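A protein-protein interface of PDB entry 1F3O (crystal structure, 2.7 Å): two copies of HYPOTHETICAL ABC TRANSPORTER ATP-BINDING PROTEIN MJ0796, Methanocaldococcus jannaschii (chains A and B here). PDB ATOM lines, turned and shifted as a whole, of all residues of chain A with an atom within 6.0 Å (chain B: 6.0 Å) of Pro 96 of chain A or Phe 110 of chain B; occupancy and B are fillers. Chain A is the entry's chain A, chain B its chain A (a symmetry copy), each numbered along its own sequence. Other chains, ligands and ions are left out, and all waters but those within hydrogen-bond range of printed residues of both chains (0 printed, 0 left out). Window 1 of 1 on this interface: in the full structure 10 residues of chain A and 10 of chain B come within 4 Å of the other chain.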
ATOM      1  N   LEU A  94      19.359 -21.084   7.000  1.00  0.00           N
ATOM      2  CA  LEU A  94      20.710 -21.107   7.550  1.00  0.00           C
ATOM      3  C   LEU A  94      21.677 -20.245   6.735  1.00  0.00           C
ATOM      4  O   LEU A  94      21.438 -20.032   5.549  1.00  0.00           O
ATOM      5  CB  LEU A  94      21.208 -22.543   7.581  1.00  0.00           C
ATOM      6  CG  LEU A  94      20.392 -23.555   8.393  1.00  0.00           C
ATOM      7  CD1 LEU A  94      21.049 -24.911   8.278  1.00  0.00           C
ATOM      8  CD2 LEU A  94      20.264 -23.146   9.848  1.00  0.00           C
ATOM      9  N   ILE A  95      22.738 -19.732   7.371  1.00  0.00           N
ATOM     10  CA  ILE A  95      23.734 -18.905   6.686  1.00  0.00           C
ATOM     11  C   ILE A  95      24.702 -19.902   6.087  1.00  0.00           C
ATOM     12  O   ILE A  95      25.261 -20.708   6.832  1.00  0.00           O
ATOM     13  CB  ILE A  95      24.448 -17.961   7.659  1.00  0.00           C
ATOM     14  CG1 ILE A  95      23.556 -16.771   7.980  1.00  0.00           C
ATOM     15  CG2 ILE A  95      25.633 -17.354   7.008  1.00  0.00           C
ATOM     16  CD1 ILE A  95      22.253 -17.129   8.556  1.00  0.00           C
ATOM     17  N   PRO A  96      24.864 -19.893   4.731  1.00  0.00           N
ATOM     18  CA  PRO A  96      25.730 -20.775   3.930  1.00  0.00           C
ATOM     19  C   PRO A  96      27.226 -20.932   4.235  1.00  0.00           C
ATOM     20  O   PRO A  96      27.822 -21.997   3.980  1.00  0.00           O
ATOM     21  CB  PRO A  96      25.460 -20.314   2.484  1.00  0.00           C
ATOM     22  CG  PRO A  96      24.919 -18.949   2.622  1.00  0.00           C
ATOM     23  CD  PRO A  96      24.078 -19.005   3.840  1.00  0.00           C
ATOM     24  N   LEU A  97      27.811 -19.897   4.827  1.00  0.00           N
ATOM     25  CA  LEU A  97      29.230 -19.889   5.164  1.00  0.00           C
ATOM     26  C   LEU A  97      29.521 -20.067   6.633  1.00  0.00           C
ATOM     27  O   LEU A  97      30.610 -19.757   7.079  1.00  0.00           O
ATOM     28  CB  LEU A  97      29.857 -18.596   4.684  1.00  0.00           C
ATOM     29  CG  LEU A  97      29.873 -18.461   3.157  1.00  0.00           C
ATOM     30  CD1 LEU A  97      30.169 -17.024   2.753  1.00  0.00           C
ATOM     31  CD2 LEU A  97      30.874 -19.445   2.543  1.00  0.00           C
ATOM     32  N   LEU A  98      28.532 -20.533   7.384  1.00  0.00           N
ATOM     33  CA  LEU A  98      28.701 -20.778   8.797  1.00  0.00           C
ATOM     34  C   LEU A  98      28.416 -22.232   9.100  1.00  0.00           C
ATOM     35  O   LEU A  98      27.484 -22.848   8.571  1.00  0.00           O
ATOM     36  CB  LEU A  98      27.800 -19.878   9.658  1.00  0.00           C
ATOM     37  CG  LEU A  98      28.190 -18.413   9.868  1.00  0.00           C
ATOM     38  CD1 LEU A  98      27.324 -17.763  10.945  1.00  0.00           C
ATOM     39  CD2 LEU A  98      29.637 -18.333  10.250  1.00  0.00           C
ATOM     40  N   ASN A 103      25.865 -21.320  13.227  1.00  0.00           N
ATOM     41  CA  ASN A 103      24.499 -20.858  12.985  1.00  0.00           C
ATOM     42  C   ASN A 103      23.684 -20.830  14.280  1.00  0.00           C
ATOM     43  O   ASN A 103      22.762 -20.033  14.423  1.00  0.00           O
ATOM     44  CB  ASN A 103      23.823 -21.734  11.937  1.00  0.00           C
ATOM     45  CG  ASN A 103      24.185 -21.335  10.537  1.00  0.00           C
ATOM     46  OD1 ASN A 103      23.669 -20.370  10.023  1.00  0.00           O
ATOM     47  ND2 ASN A 103      25.073 -22.078   9.909  1.00  0.00           N
ATOM     48  N   LYS A 142      28.983 -27.399   7.416  1.00  0.00           N
ATOM     49  CA  LYS A 142      28.224 -26.248   6.989  1.00  0.00           C
ATOM     50  C   LYS A 142      26.922 -26.778   6.387  1.00  0.00           C
ATOM     51  O   LYS A 142      26.806 -27.992   6.141  1.00  0.00           O
ATOM     52  CB  LYS A 142      29.050 -25.377   6.041  1.00  0.00           C
ATOM     53  CG  LYS A 142      30.351 -24.871   6.659  1.00  0.00           C
ATOM     54  CD  LYS A 142      30.975 -23.739   5.827  1.00  0.00           C
ATOM     55  CE  LYS A 142      32.319 -23.296   6.407  1.00  0.00           C
ATOM     56  NZ  LYS A 142      32.102 -22.796   7.784  1.00  0.00           N
ATOM     57  N   PRO A 143      25.974 -25.880   6.058  1.00  0.00           N
ATOM     58  CA  PRO A 143      24.672 -26.191   5.489  1.00  0.00           C
ATOM     59  C   PRO A 143      24.596 -27.314   4.456  1.00  0.00           C
ATOM     60  O   PRO A 143      24.255 -28.434   4.803  1.00  0.00           O
ATOM     61  CB  PRO A 143      24.203 -24.869   4.920  1.00  0.00           C
ATOM     62  CG  PRO A 143      24.976 -23.876   5.677  1.00  0.00           C
ATOM     63  CD  PRO A 143      26.297 -24.480   5.737  1.00  0.00           C
ATOM     64  N   ASN A 144      25.005 -26.998   3.237  1.00  0.00           N
ATOM     65  CA  ASN A 144      24.994 -27.924   2.104  1.00  0.00           C
ATOM     66  C   ASN A 144      25.700 -29.268   2.274  1.00  0.00           C
ATOM     67  O   ASN A 144      25.795 -30.053   1.312  1.00  0.00           O
ATOM     68  CB  ASN A 144      25.594 -27.218   0.894  1.00  0.00           C
ATOM     69  CG  ASN A 144      27.097 -27.027   1.018  1.00  0.00           C
ATOM     70  OD1 ASN A 144      27.565 -26.210   1.801  1.00  0.00           O
ATOM     71  ND2 ASN A 144      27.856 -27.820   0.278  1.00  0.00           N
ATOM     72  N   ARG B  82      16.573  -8.206  -4.905  1.00  0.00           N
ATOM     73  CA  ARG B  82      17.881  -8.819  -5.058  1.00  0.00           C
ATOM     74  C   ARG B  82      18.614  -8.445  -6.316  1.00  0.00           C
ATOM     75  O   ARG B  82      19.833  -8.565  -6.367  1.00  0.00           O
ATOM     76  CB  ARG B  82      17.784 -10.342  -4.968  1.00  0.00           C
ATOM     77  CG  ARG B  82      17.296 -10.891  -3.616  1.00  0.00           C
ATOM     78  CD  ARG B  82      17.491 -12.420  -3.512  1.00  0.00           C
ATOM     79  NE  ARG B  82      16.844 -13.007  -2.339  1.00  0.00           N
ATOM     80  CZ  ARG B  82      17.049 -14.251  -1.916  1.00  0.00           C
ATOM     81  NH1 ARG B  82      17.892 -15.052  -2.562  1.00  0.00           N
ATOM     82  NH2 ARG B  82      16.380 -14.711  -0.861  1.00  0.00           N
ATOM     83  N   GLU B 105      30.003 -11.951   0.098  1.00  0.00           N
ATOM     84  CA  GLU B 105      29.707 -13.144  -0.695  1.00  0.00           C
ATOM     85  C   GLU B 105      28.235 -13.629  -0.561  1.00  0.00           C
ATOM     86  O   GLU B 105      27.608 -14.032  -1.535  1.00  0.00           O
ATOM     87  CB  GLU B 105      30.677 -14.272  -0.324  1.00  0.00           C
ATOM     88  CG  GLU B 105      32.057 -14.150  -0.924  1.00  0.00           C
ATOM     89  CD  GLU B 105      32.949 -15.262  -0.460  1.00  0.00           C
ATOM     90  OE1 GLU B 105      33.769 -14.957   0.438  1.00  0.00           O
ATOM     91  OE2 GLU B 105      32.812 -16.422  -0.959  1.00  0.00           O
ATOM     92  N   LEU B 106      27.688 -13.558   0.642  1.00  0.00           N
ATOM     93  CA  LEU B 106      26.322 -13.964   0.907  1.00  0.00           C
ATOM     94  C   LEU B 106      25.287 -13.610  -0.166  1.00  0.00           C
ATOM     95  O   LEU B 106      24.639 -14.528  -0.689  1.00  0.00           O
ATOM     96  CB  LEU B 106      25.861 -13.415   2.257  1.00  0.00           C
ATOM     97  CG  LEU B 106      26.170 -14.179   3.535  1.00  0.00           C
ATOM     98  CD1 LEU B 106      25.576 -13.453   4.733  1.00  0.00           C
ATOM     99  CD2 LEU B 106      25.519 -15.528   3.409  1.00  0.00           C
ATOM    100  N   PRO B 107      25.114 -12.295  -0.521  1.00  0.00           N
ATOM    101  CA  PRO B 107      24.119 -11.928  -1.545  1.00  0.00           C
ATOM    102  C   PRO B 107      24.366 -12.614  -2.866  1.00  0.00           C
ATOM    103  O   PRO B 107      23.430 -12.926  -3.577  1.00  0.00           O
ATOM    104  CB  PRO B 107      24.286 -10.417  -1.708  1.00  0.00           C
ATOM    105  CG  PRO B 107      25.147  -9.974  -0.637  1.00  0.00           C
ATOM    106  CD  PRO B 107      25.859 -11.104  -0.050  1.00  0.00           C
ATOM    107  N   LEU B 108      25.630 -12.829  -3.187  1.00  0.00           N
ATOM    108  CA  LEU B 108      26.010 -13.492  -4.419  1.00  0.00           C
ATOM    109  C   LEU B 108      25.666 -14.979  -4.377  1.00  0.00           C
ATOM    110  O   LEU B 108      25.395 -15.578  -5.422  1.00  0.00           O
ATOM    111  CB  LEU B 108      27.492 -13.299  -4.679  1.00  0.00           C
ATOM    112  CG  LEU B 108      27.981 -11.872  -4.947  1.00  0.00           C
ATOM    113  CD1 LEU B 108      29.526 -11.817  -5.095  1.00  0.00           C
ATOM    114  CD2 LEU B 108      27.321 -11.362  -6.184  1.00  0.00           C
ATOM    115  N   ILE B 109      25.652 -15.562  -3.176  1.00  0.00           N
ATOM    116  CA  ILE B 109      25.285 -16.974  -2.973  1.00  0.00           C
ATOM    117  C   ILE B 109      23.796 -17.135  -3.236  1.00  0.00           C
ATOM    118  O   ILE B 109      23.356 -18.038  -3.945  1.00  0.00           O
ATOM    119  CB  ILE B 109      25.483 -17.415  -1.524  1.00  0.00           C
ATOM    120  CG1 ILE B 109      26.897 -17.117  -1.068  1.00  0.00           C
ATOM    121  CG2 ILE B 109      25.191 -18.870  -1.402  1.00  0.00           C
ATOM    122  CD1 ILE B 109      27.247 -17.743   0.243  1.00  0.00           C
ATOM    123  N   PHE B 110      23.033 -16.209  -2.672  1.00  0.00           N
ATOM    124  CA  PHE B 110      21.586 -16.171  -2.777  1.00  0.00           C
ATOM    125  C   PHE B 110      21.021 -15.890  -4.162  1.00  0.00           C
ATOM    126  O   PHE B 110      19.858 -16.233  -4.416  1.00  0.00           O
ATOM    127  CB  PHE B 110      21.023 -15.195  -1.754  1.00  0.00           C
ATOM    128  CG  PHE B 110      21.401 -15.532  -0.346  1.00  0.00           C
ATOM    129  CD1 PHE B 110      21.754 -14.535   0.569  1.00  0.00           C
ATOM    130  CD2 PHE B 110      21.394 -16.872   0.095  1.00  0.00           C
ATOM    131  CE1 PHE B 110      22.100 -14.864   1.925  1.00  0.00           C
ATOM    132  CE2 PHE B 110      21.740 -17.235   1.456  1.00  0.00           C
ATOM    133  CZ  PHE B 110      22.093 -16.222   2.372  1.00  0.00           C
ATOM    134  N   LYS B 111      21.824 -15.281  -5.036  1.00  0.00           N
ATOM    135  CA  LYS B 111      21.405 -14.961  -6.394  1.00  0.00           C
ATOM    136  C   LYS B 111      21.914 -15.962  -7.392  1.00  0.00           C
ATOM    137  O   LYS B 111      21.189 -16.367  -8.286  1.00  0.00           O
ATOM    138  CB  LYS B 111      21.892 -13.567  -6.819  1.00  0.00           C
ATOM    139  CG  LYS B 111      21.712 -13.284  -8.356  1.00  0.00           C
ATOM    140  CD  LYS B 111      22.289 -11.938  -8.849  1.00  0.00           C
ATOM    141  CE  LYS B 111      22.072 -11.783 -10.345  1.00  0.00           C
ATOM    142  NZ  LYS B 111      22.752 -10.508 -10.787  1.00  0.00           N
ATOM    143  N   TYR B 112      23.179 -16.327  -7.244  1.00  0.00           N
ATOM    144  CA  TYR B 112      23.860 -17.238  -8.148  1.00  0.00           C
ATOM    145  C   TYR B 112      24.159 -18.597  -7.559  1.00  0.00           C
ATOM    146  O   TYR B 112      25.225 -19.131  -7.832  1.00  0.00           O
ATOM    147  CB  TYR B 112      25.208 -16.652  -8.546  1.00  0.00           C
ATOM    148  CG  TYR B 112      25.208 -15.237  -9.000  1.00  0.00           C
ATOM    149  CD1 TYR B 112      25.261 -14.184  -8.083  1.00  0.00           C
ATOM    150  CD2 TYR B 112      25.231 -14.928 -10.346  1.00  0.00           C
ATOM    151  CE1 TYR B 112      25.340 -12.868  -8.490  1.00  0.00           C
ATOM    152  CE2 TYR B 112      25.306 -13.618 -10.776  1.00  0.00           C
ATOM    153  CZ  TYR B 112      25.359 -12.577  -9.836  1.00  0.00           C
ATOM    154  OH  TYR B 112      25.397 -11.244 -10.225  1.00  0.00           O
ATOM    155  N   ARG B 113      23.260 -19.201  -6.805  1.00  0.00           N
ATOM    156  CA  ARG B 113      23.598 -20.498  -6.245  1.00  0.00           C
ATOM    157  C   ARG B 113      23.848 -21.594  -7.272  1.00  0.00           C
ATOM    158  O   ARG B 113      23.053 -21.811  -8.195  1.00  0.00           O
ATOM    159  CB  ARG B 113      22.554 -20.918  -5.223  1.00  0.00           C
ATOM    160  CG  ARG B 113      21.155 -20.960  -5.750  1.00  0.00           C
ATOM    161  CD  ARG B 113      20.179 -21.095  -4.608  1.00  0.00           C
ATOM    162  NE  ARG B 113      18.857 -21.574  -5.032  1.00  0.00           N
ATOM    163  CZ  ARG B 113      17.847 -21.799  -4.189  1.00  0.00           C
ATOM    164  NH1 ARG B 113      18.005 -21.573  -2.887  1.00  0.00           N
ATOM    165  NH2 ARG B 113      16.689 -22.284  -4.638  1.00  0.00           N
ATOM    166  N   ARG B 121      33.259 -15.891  -6.635  1.00  0.00           N
ATOM    167  CA  ARG B 121      32.590 -15.151  -5.559  1.00  0.00           C
ATOM    168  C   ARG B 121      33.638 -14.402  -4.782  1.00  0.00           C
ATOM    169  O   ARG B 121      33.426 -13.250  -4.471  1.00  0.00           O
ATOM    170  CB  ARG B 121      31.917 -16.057  -4.551  1.00  0.00           C
ATOM    171  CG  ARG B 121      30.605 -16.644  -4.924  1.00  0.00           C
ATOM    172  CD  ARG B 121      30.165 -17.623  -3.837  1.00  0.00           C
ATOM    173  NE  ARG B 121      29.026 -18.436  -4.241  1.00  0.00           N
ATOM    174  CZ  ARG B 121      28.257 -19.117  -3.399  1.00  0.00           C
ATOM    175  NH1 ARG B 121      28.515 -19.105  -2.099  1.00  0.00           N
ATOM    176  NH2 ARG B 121      27.164 -19.723  -3.841  1.00  0.00           N
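O of Leu 97 of chain A is in hydrogen-bond range of NZ of Lys 142 of chain A, at 3.5 Å. O of Phe 110 of chain B lies within hydrogen-bond range of NH1 of Arg 82 of chain B (2.9 Å).
Among the printed residues, merely in contact across the chains: Pro 96 of chain A with Leu 106 of chain B, Pro 96 of chain A with Ile 109 of chain B, Pro 96 of chain A with Phe 110 of chain B and Leu 97 of chain A with Ile 109 of chain B.
Pro 96 of chain A touches just these residues of chain B: Leu 106 (3.6 Å), Ile 109 (3.5 Å) and Phe 110 (3.7 Å). Of chain A, only Pro 96 comes within 4 Å of Phe 110 of chain B. Printed residues of chain B within 4 Å of Leu 97 of chain A: Ile 109 (3.9 Å). Printed residues of chain A within 4 Å of Leu 106 of chain B: Pro 96 (3.6 Å). Asn 144 of chain A touches none of the printed residues of chain B. Pro 107 of chain B touches none of the printed residues of chain A.
Of the 9 printed residues of chain A, 2 touch a printed residue of chain B. Hydrophobic or aromatic side chains of chain B that line the printed part of chain A: Leu 106, Ile 109 and Phe 110. Among the printed residues, 4 pairs touch across the chains.
No position is printed for both chains.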
